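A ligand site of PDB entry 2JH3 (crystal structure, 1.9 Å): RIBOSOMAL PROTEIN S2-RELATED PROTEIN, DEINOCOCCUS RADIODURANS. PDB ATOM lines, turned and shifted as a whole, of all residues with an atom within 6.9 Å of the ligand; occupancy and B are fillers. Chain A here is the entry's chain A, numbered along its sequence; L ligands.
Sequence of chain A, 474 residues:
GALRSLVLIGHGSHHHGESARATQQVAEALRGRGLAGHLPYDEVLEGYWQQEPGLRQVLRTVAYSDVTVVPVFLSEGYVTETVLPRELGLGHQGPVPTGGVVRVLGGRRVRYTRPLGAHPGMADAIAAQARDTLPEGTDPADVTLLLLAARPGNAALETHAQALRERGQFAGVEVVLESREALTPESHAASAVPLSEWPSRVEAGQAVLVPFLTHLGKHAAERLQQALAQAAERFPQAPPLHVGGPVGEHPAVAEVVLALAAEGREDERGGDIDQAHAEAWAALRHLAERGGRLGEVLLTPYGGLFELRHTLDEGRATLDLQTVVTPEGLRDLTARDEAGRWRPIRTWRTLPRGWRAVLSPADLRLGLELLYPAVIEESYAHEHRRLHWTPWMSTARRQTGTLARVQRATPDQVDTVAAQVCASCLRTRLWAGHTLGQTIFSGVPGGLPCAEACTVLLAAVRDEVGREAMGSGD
The side-chain sulfur of Cys 422 is bound to an iron atom (FE4) of the ligand (2.4 Å). SG of Cys 454 is bound to FE2 of the ligand, 2.4 Å away. NE1 of Trp 348 sits close to S1 of the ligand, at 3.4 Å. An iron atom (FE1) of the ligand is bound by the side-chain sulfur of Cys 450 (2.3 Å). The backbone NH (N) of Cys 454 sits close to a sulfur (S3) of the ligand, 3.5 Å away. SG of Cys 425 is bound to FE3 of the ligand (2.3 Å).
The backbone carbonyl oxygen of Pro 449 lies within hydrogen-bond range of the guanidinium group of Arg 427 (3.3 Å). The backbone NH (N) of Cys 450 is in hydrogen-bond range of the backbone carbonyl oxygen (O) of Thr 428. The side-chain sulfur (SG) of Cys 422 lies close to the backbone carbonyl oxygen (O) of Ala 418 (3.3 Å). The side-chain sulfur of Cys 454 lies close to the backbone NH of Leu 457, at 3.6 Å. The side-chain sulfur (SG) of Cys 450 lies close to the indole nitrogen (NE1) of Trp 431. The side-chain sulfur (SG) of Cys 450 lies close to the backbone carbonyl oxygen (O) of Glu 452 (3.2 Å). The backbone carbonyl oxygen of Cys 450 sits at hydrogen-bond distance from the backbone NH of Leu 430, 3.0 Å away. SG of Cys 425 sits close to OG1 of Thr 347.
CB of Arg 427 touches S2 of the ligand (3.8 Å). CZ2 of Trp 431 touches S3 of the ligand (3.99 Å). Ala 453 touches the ligand. Leu 457 touches the ligand (CD2 to S3, 3.7 Å). Hydrophobic or aromatic side chains that line the ligand: Trp 431 and Leu 457. Nine residues have an atom within 4 Å of the ligand: Trp 348, Cys 422, Cys 425, Arg 427, Trp 431, Cys 450, Ala 453, Cys 454 and Leu 457. The nearest printed residue that does not touch the ligand is Glu 452 (4.1 Å).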
ATOM      1  N   GLU A  52     -12.776   1.198  24.381  1.00  0.00           N
ATOM      2  CA  GLU A  52     -14.022   0.785  23.722  1.00  0.00           C
ATOM      3  C   GLU A  52     -15.224   1.161  24.599  1.00  0.00           C
ATOM      4  O   GLU A  52     -15.137   1.057  25.832  1.00  0.00           O
ATOM      5  CB  GLU A  52     -14.017  -0.718  23.469  1.00  0.00           C
ATOM      6  CG  GLU A  52     -12.991  -1.156  22.464  1.00  0.00           C
ATOM      7  CD  GLU A  52     -13.258  -2.606  22.010  1.00  0.00           C
ATOM      8  OE1 GLU A  52     -13.579  -3.512  22.870  1.00  0.00           O
ATOM      9  OE2 GLU A  52     -13.193  -2.786  20.769  1.00  0.00           O
ATOM     10  N   GLN A  57     -15.956   3.088  16.273  1.00  0.00           N
ATOM     11  CA  GLN A  57     -16.971   2.052  16.430  1.00  0.00           C
ATOM     12  C   GLN A  57     -18.324   2.685  16.684  1.00  0.00           C
ATOM     13  O   GLN A  57     -19.358   2.165  16.274  1.00  0.00           O
ATOM     14  CB  GLN A  57     -16.588   1.181  17.646  1.00  0.00           C
ATOM     15  CG  GLN A  57     -15.214   0.549  17.572  1.00  0.00           C
ATOM     16  CD  GLN A  57     -15.010  -0.365  18.775  1.00  0.00           C
ATOM     17  OE1 GLN A  57     -15.365   0.022  19.916  1.00  0.00           O
ATOM     18  NE2 GLN A  57     -14.593  -1.605  18.534  1.00  0.00           N
ATOM     19  N   ILE A 345      -9.810  -2.708  25.844  1.00  0.00           N
ATOM     20  CA  ILE A 345     -10.246  -3.475  24.736  1.00  0.00           C
ATOM     21  C   ILE A 345     -10.997  -4.705  25.242  1.00  0.00           C
ATOM     22  O   ILE A 345     -10.400  -5.615  25.797  1.00  0.00           O
ATOM     23  CB  ILE A 345      -9.028  -3.938  23.823  1.00  0.00           C
ATOM     24  CG1 ILE A 345      -8.140  -2.773  23.381  1.00  0.00           C
ATOM     25  CG2 ILE A 345      -9.566  -4.680  22.643  1.00  0.00           C
ATOM     26  CD1 ILE A 345      -8.815  -1.633  22.627  1.00  0.00           C
ATOM     27  N   THR A 347     -12.743  -7.148  23.934  1.00  0.00           N
ATOM     28  CA  THR A 347     -12.538  -8.465  23.302  1.00  0.00           C
ATOM     29  C   THR A 347     -11.235  -9.217  23.714  1.00  0.00           C
ATOM     30  O   THR A 347     -10.964 -10.265  23.197  1.00  0.00           O
ATOM     31  CB  THR A 347     -12.541  -8.362  21.818  1.00  0.00           C
ATOM     32  OG1 THR A 347     -11.681  -7.313  21.341  1.00  0.00           O
ATOM     33  CG2 THR A 347     -13.950  -8.089  21.345  1.00  0.00           C
ATOM     34  N   TRP A 348     -10.459  -8.643  24.618  1.00  0.00           N
ATOM     35  CA  TRP A 348      -9.330  -9.343  25.180  1.00  0.00           C
ATOM     36  C   TRP A 348      -9.818 -10.519  25.981  1.00  0.00           C
ATOM     37  O   TRP A 348     -10.885 -10.464  26.598  1.00  0.00           O
ATOM     38  CB  TRP A 348      -8.389  -8.403  25.977  1.00  0.00           C
ATOM     39  CG  TRP A 348      -7.440  -7.737  25.062  1.00  0.00           C
ATOM     40  CD1 TRP A 348      -7.691  -7.382  23.762  1.00  0.00           C
ATOM     41  CD2 TRP A 348      -6.140  -7.279  25.362  1.00  0.00           C
ATOM     42  NE1 TRP A 348      -6.585  -6.797  23.227  1.00  0.00           N
ATOM     43  CE2 TRP A 348      -5.607  -6.752  24.188  1.00  0.00           C
ATOM     44  CE3 TRP A 348      -5.313  -7.392  26.496  1.00  0.00           C
ATOM     45  CZ2 TRP A 348      -4.308  -6.206  24.122  1.00  0.00           C
ATOM     46  CZ3 TRP A 348      -4.030  -6.910  26.427  1.00  0.00           C
ATOM     47  CH2 TRP A 348      -3.530  -6.328  25.249  1.00  0.00           C
ATOM     48  N   ALA A 418       1.992  -6.629  16.411  1.00  0.00           N
ATOM     49  CA  ALA A 418       0.642  -7.133  16.360  1.00  0.00           C
ATOM     50  C   ALA A 418       0.574  -8.596  16.785  1.00  0.00           C
ATOM     51  O   ALA A 418      -0.326  -8.980  17.528  1.00  0.00           O
ATOM     52  CB  ALA A 418       0.080  -6.930  15.031  1.00  0.00           C
ATOM     53  N   VAL A 421       0.781  -8.310  20.683  1.00  0.00           N
ATOM     54  CA  VAL A 421      -0.367  -7.645  21.319  1.00  0.00           C
ATOM     55  C   VAL A 421      -1.705  -8.348  21.048  1.00  0.00           C
ATOM     56  O   VAL A 421      -2.432  -8.695  21.969  1.00  0.00           O
ATOM     57  CB  VAL A 421      -0.495  -6.264  20.754  1.00  0.00           C
ATOM     58  CG1 VAL A 421      -1.834  -5.573  21.158  1.00  0.00           C
ATOM     59  CG2 VAL A 421       0.664  -5.438  21.320  1.00  0.00           C
ATOM     60  N   CYS A 422      -1.944  -8.643  19.793  1.00  0.00           N
ATOM     61  CA  CYS A 422      -3.208  -9.208  19.374  1.00  0.00           C
ATOM     62  C   CYS A 422      -3.465 -10.640  19.871  1.00  0.00           C
ATOM     63  O   CYS A 422      -4.607 -11.129  19.869  1.00  0.00           O
ATOM     64  CB  CYS A 422      -3.332  -9.153  17.870  1.00  0.00           C
ATOM     65  SG  CYS A 422      -3.302  -7.493  17.168  1.00  0.00           S
ATOM     66  N   ALA A 423      -2.377 -11.312  20.300  1.00  0.00           N
ATOM     67  CA  ALA A 423      -2.522 -12.625  20.933  1.00  0.00           C
ATOM     68  C   ALA A 423      -3.400 -12.649  22.128  1.00  0.00           C
ATOM     69  O   ALA A 423      -3.938 -13.712  22.517  1.00  0.00           O
ATOM     70  CB  ALA A 423      -1.173 -13.186  21.253  1.00  0.00           C
ATOM     71  N   SER A 424      -3.545 -11.498  22.779  1.00  0.00           N
ATOM     72  CA  SER A 424      -4.462 -11.378  23.902  1.00  0.00           C
ATOM     73  C   SER A 424      -5.913 -11.213  23.526  1.00  0.00           C
ATOM     74  O   SER A 424      -6.806 -11.307  24.397  1.00  0.00           O
ATOM     75  CB  SER A 424      -4.020 -10.207  24.785  1.00  0.00           C
ATOM     76  OG  SER A 424      -2.844 -10.558  25.522  1.00  0.00           O
ATOM     77  N   CYS A 425      -6.165 -10.959  22.247  1.00  0.00           N
ATOM     78  CA  CYS A 425      -7.449 -10.539  21.757  1.00  0.00           C
ATOM     79  C   CYS A 425      -8.237 -11.690  21.151  1.00  0.00           C
ATOM     80  O   CYS A 425      -7.654 -12.560  20.491  1.00  0.00           O
ATOM     81  CB  CYS A 425      -7.234  -9.477  20.666  1.00  0.00           C
ATOM     82  SG  CYS A 425      -8.700  -8.468  20.321  1.00  0.00           S
ATOM     83  N   LEU A 426      -9.547 -11.699  21.307  1.00  0.00           N
ATOM     84  CA  LEU A 426     -10.428 -12.636  20.544  1.00  0.00           C
ATOM     85  C   LEU A 426     -10.505 -12.426  19.015  1.00  0.00           C
ATOM     86  O   LEU A 426     -10.868 -13.320  18.212  1.00  0.00           O
ATOM     87  CB  LEU A 426     -11.828 -12.541  21.104  1.00  0.00           C
ATOM     88  CG  LEU A 426     -12.362 -13.446  22.266  1.00  0.00           C
ATOM     89  CD1 LEU A 426     -11.408 -14.286  22.936  1.00  0.00           C
ATOM     90  CD2 LEU A 426     -13.391 -12.769  23.225  1.00  0.00           C
ATOM     91  N   ARG A 427     -10.296 -11.199  18.623  1.00  0.00           N
ATOM     92  CA  ARG A 427     -10.539 -10.789  17.249  1.00  0.00           C
ATOM     93  C   ARG A 427      -9.445 -11.255  16.304  1.00  0.00           C
ATOM     94  O   ARG A 427      -8.323 -11.636  16.741  1.00  0.00           O
ATOM     95  CB  ARG A 427     -10.678  -9.263  17.185  1.00  0.00           C
ATOM     96  CG  ARG A 427     -11.913  -8.753  17.822  1.00  0.00           C
ATOM     97  CD  ARG A 427     -11.993  -7.255  17.611  1.00  0.00           C
ATOM     98  NE  ARG A 427     -13.333  -6.620  17.791  1.00  0.00           N
ATOM     99  CZ  ARG A 427     -13.687  -5.716  18.684  1.00  0.00           C
ATOM    100  NH1 ARG A 427     -14.870  -5.130  18.588  1.00  0.00           N
ATOM    101  NH2 ARG A 427     -12.833  -5.270  19.595  1.00  0.00           N
ATOM    102  N   THR A 428      -9.808 -11.266  15.014  1.00  0.00           N
ATOM    103  CA  THR A 428      -8.943 -11.631  13.871  1.00  0.00           C
ATOM    104  C   THR A 428      -8.727 -10.361  13.013  1.00  0.00           C
ATOM    105  O   THR A 428      -9.681  -9.777  12.525  1.00  0.00           O
ATOM    106  CB  THR A 428      -9.632 -12.734  12.983  1.00  0.00           C
ATOM    107  OG1 THR A 428      -9.776 -13.956  13.725  1.00  0.00           O
ATOM    108  CG2 THR A 428      -8.787 -13.077  11.752  1.00  0.00           C
ATOM    109  N   ARG A 429      -7.461  -9.961  12.889  1.00  0.00           N
ATOM    110  CA  ARG A 429      -7.051  -8.693  12.197  1.00  0.00           C
ATOM    111  C   ARG A 429      -7.190  -8.755  10.707  1.00  0.00           C
ATOM    112  O   ARG A 429      -6.249  -9.005   9.971  1.00  0.00           O
ATOM    113  CB  ARG A 429      -5.659  -8.246  12.677  1.00  0.00           C
ATOM    114  CG  ARG A 429      -4.546  -9.240  12.553  1.00  0.00           C
ATOM    115  CD  ARG A 429      -3.337  -8.728  13.338  1.00  0.00           C
ATOM    116  NE  ARG A 429      -2.131  -9.580  13.263  1.00  0.00           N
ATOM    117  CZ  ARG A 429      -1.924 -10.627  14.056  1.00  0.00           C
ATOM    118  NH1 ARG A 429      -0.781 -11.286  13.977  1.00  0.00           N
ATOM    119  NH2 ARG A 429      -2.832 -11.008  14.975  1.00  0.00           N
ATOM    120  N   LEU A 430      -8.384  -8.462  10.243  1.00  0.00           N
ATOM    121  CA  LEU A 430      -8.710  -8.428   8.826  1.00  0.00           C
ATOM    122  C   LEU A 430      -7.841  -7.424   8.061  1.00  0.00           C
ATOM    123  O   LEU A 430      -7.498  -7.609   6.877  1.00  0.00           O
ATOM    124  CB  LEU A 430     -10.145  -7.998   8.693  1.00  0.00           C
ATOM    125  CG  LEU A 430     -11.241  -9.037   8.468  1.00  0.00           C
ATOM    126  CD1 LEU A 430     -10.970 -10.459   8.937  1.00  0.00           C
ATOM    127  CD2 LEU A 430     -12.583  -8.446   8.863  1.00  0.00           C
ATOM    128  N   TRP A 431      -7.476  -6.370   8.773  1.00  0.00           N
ATOM    129  CA  TRP A 431      -6.742  -5.255   8.206  1.00  0.00           C
ATOM    130  C   TRP A 431      -5.299  -5.652   7.909  1.00  0.00           C
ATOM    131  O   TRP A 431      -4.590  -4.925   7.250  1.00  0.00           O
ATOM    132  CB  TRP A 431      -6.788  -4.054   9.144  1.00  0.00           C
ATOM    133  CG  TRP A 431      -6.257  -4.331  10.598  1.00  0.00           C
ATOM    134  CD1 TRP A 431      -7.035  -4.638  11.665  1.00  0.00           C
ATOM    135  CD2 TRP A 431      -4.920  -4.288  11.071  1.00  0.00           C
ATOM    136  NE1 TRP A 431      -6.265  -4.873  12.767  1.00  0.00           N
ATOM    137  CE2 TRP A 431      -4.960  -4.614  12.451  1.00  0.00           C
ATOM    138  CE3 TRP A 431      -3.669  -3.982  10.485  1.00  0.00           C
ATOM    139  CZ2 TRP A 431      -3.810  -4.689  13.246  1.00  0.00           C
ATOM    140  CZ3 TRP A 431      -2.533  -3.997  11.301  1.00  0.00           C
ATOM    141  CH2 TRP A 431      -2.607  -4.352  12.655  1.00  0.00           C
ATOM    142  N   PRO A 449     -14.422 -10.461  14.075  1.00  0.00           N
ATOM    143  CA  PRO A 449     -13.483  -9.621  13.272  1.00  0.00           C
ATOM    144  C   PRO A 449     -12.931  -8.367  13.902  1.00  0.00           C
ATOM    145  O   PRO A 449     -13.573  -7.713  14.731  1.00  0.00           O
ATOM    146  CB  PRO A 449     -14.328  -9.243  12.058  1.00  0.00           C
ATOM    147  CG  PRO A 449     -15.789  -9.276  12.562  1.00  0.00           C
ATOM    148  CD  PRO A 449     -15.845 -10.298  13.657  1.00  0.00           C
ATOM    149  N   CYS A 450     -11.707  -8.012  13.494  1.00  0.00           N
ATOM    150  CA  CYS A 450     -11.056  -6.761  13.828  1.00  0.00           C
ATOM    151  C   CYS A 450     -10.891  -5.984  12.526  1.00  0.00           C
ATOM    152  O   CYS A 450     -10.215  -6.465  11.581  1.00  0.00           O
ATOM    153  CB  CYS A 450      -9.686  -6.909  14.489  1.00  0.00           C
ATOM    154  SG  CYS A 450      -8.959  -5.285  14.812  1.00  0.00           S
ATOM    155  N   ALA A 451     -11.554  -4.809  12.446  1.00  0.00           N
ATOM    156  CA  ALA A 451     -11.624  -4.066  11.210  1.00  0.00           C
ATOM    157  C   ALA A 451     -10.544  -2.988  11.147  1.00  0.00           C
ATOM    158  O   ALA A 451     -10.362  -2.353  10.090  1.00  0.00           O
ATOM    159  CB  ALA A 451     -13.046  -3.433  11.054  1.00  0.00           C
ATOM    160  N   GLU A 452      -9.819  -2.756  12.262  1.00  0.00           N
ATOM    161  CA  GLU A 452      -8.881  -1.603  12.305  1.00  0.00           C
ATOM    162  C   GLU A 452      -7.996  -1.746  13.557  1.00  0.00           C
ATOM    163  O   GLU A 452      -8.480  -2.160  14.640  1.00  0.00           O
ATOM    164  CB  GLU A 452      -9.627  -0.240  12.306  1.00  0.00           C
ATOM    165  CG  GLU A 452      -8.634   0.913  12.140  1.00  0.00           C
ATOM    166  CD  GLU A 452      -9.245   2.249  12.013  1.00  0.00           C
ATOM    167  OE1 GLU A 452     -10.461   2.356  12.156  1.00  0.00           O
ATOM    168  OE2 GLU A 452      -8.492   3.163  11.713  1.00  0.00           O
ATOM    169  N   ALA A 453      -6.709  -1.435  13.410  1.00  0.00           N
ATOM    170  CA  ALA A 453      -5.828  -1.362  14.495  1.00  0.00           C
ATOM    171  C   ALA A 453      -6.354  -0.432  15.569  1.00  0.00           C
ATOM    172  O   ALA A 453      -6.673   0.732  15.317  1.00  0.00           O
ATOM    173  CB  ALA A 453      -4.452  -0.963  14.049  1.00  0.00           C
ATOM    174  N   CYS A 454      -6.381  -0.960  16.806  1.00  0.00           N
ATOM    175  CA  CYS A 454      -6.883  -0.250  18.016  1.00  0.00           C
ATOM    176  C   CYS A 454      -5.852   0.640  18.773  1.00  0.00           C
ATOM    177  O   CYS A 454      -4.631   0.616  18.494  1.00  0.00           O
ATOM    178  CB  CYS A 454      -7.498  -1.287  19.018  1.00  0.00           C
ATOM    179  SG  CYS A 454      -6.298  -2.246  19.821  1.00  0.00           S
ATOM    180  N   THR A 455      -6.327   1.437  19.715  1.00  0.00           N
ATOM    181  CA  THR A 455      -5.417   2.373  20.390  1.00  0.00           C
ATOM    182  C   THR A 455      -4.345   1.648  21.209  1.00  0.00           C
ATOM    183  O   THR A 455      -3.266   2.151  21.340  1.00  0.00           O
ATOM    184  CB  THR A 455      -6.092   3.452  21.280  1.00  0.00           C
ATOM    185  OG1 THR A 455      -6.883   2.809  22.241  1.00  0.00           O
ATOM    186  CG2 THR A 455      -6.982   4.362  20.408  1.00  0.00           C
ATOM    187  N   VAL A 456      -4.640   0.434  21.692  1.00  0.00           N
ATOM    188  CA  VAL A 456      -3.659  -0.315  22.493  1.00  0.00           C
ATOM    189  C   VAL A 456      -2.503  -0.805  21.595  1.00  0.00           C
ATOM    190  O   VAL A 456      -1.299  -0.698  21.988  1.00  0.00           O
ATOM    191  CB  VAL A 456      -4.330  -1.422  23.287  1.00  0.00           C
ATOM    192  CG1 VAL A 456      -3.290  -2.427  23.875  1.00  0.00           C
ATOM    193  CG2 VAL A 456      -5.153  -0.832  24.457  1.00  0.00           C
ATOM    194  N   LEU A 457      -2.830  -1.279  20.389  1.00  0.00           N
ATOM    195  CA  LEU A 457      -1.812  -1.695  19.440  1.00  0.00           C
ATOM    196  C   LEU A 457      -1.002  -0.504  18.918  1.00  0.00           C
ATOM    197  O   LEU A 457       0.220  -0.623  18.777  1.00  0.00           O
ATOM    198  CB  LEU A 457      -2.446  -2.425  18.238  1.00  0.00           C
ATOM    199  CG  LEU A 457      -1.498  -2.785  17.072  1.00  0.00           C
ATOM    200  CD1 LEU A 457      -0.350  -3.674  17.602  1.00  0.00           C
ATOM    201  CD2 LEU A 457      -2.218  -3.562  15.984  1.00  0.00           C
ATOM    202  N   LEU A 458      -1.672   0.636  18.653  1.00  0.00           N
ATOM    203  CA  LEU A 458      -0.946   1.856  18.209  1.00  0.00           C
ATOM    204  C   LEU A 458       0.070   2.279  19.271  1.00  0.00           C
ATOM    205  O   LEU A 458       1.205   2.615  18.963  1.00  0.00           O
ATOM    206  CB  LEU A 458      -1.906   3.007  17.973  1.00  0.00           C
ATOM    207  CG  LEU A 458      -2.809   2.866  16.785  1.00  0.00           C
ATOM    208  CD1 LEU A 458      -3.995   3.781  16.846  1.00  0.00           C
ATOM    209  CD2 LEU A 458      -2.067   3.105  15.519  1.00  0.00           C
HETATM  210 FE1  LIG L   1      -7.723  -5.579  16.686  1.00  0.00          FE
HETATM  211 FE2  LIG L   1      -6.647  -4.396  18.873  1.00  0.00          FE
HETATM  212 FE3  LIG L   1      -7.731  -6.865  19.035  1.00  0.00          FE
HETATM  213 FE4  LIG L   1      -5.367  -6.500  17.710  1.00  0.00          FE
HETATM  214  S1  LIG L   1      -5.717  -6.179  19.985  1.00  0.00           S
HETATM  215  S2  LIG L   1      -7.146  -7.755  16.950  1.00  0.00           S
HETATM  216  S3  LIG L   1      -5.725  -4.433  16.734  1.00  0.00           S
HETATM  217  S4  LIG L   1      -8.895  -4.922  18.646  1.00  0.00           S
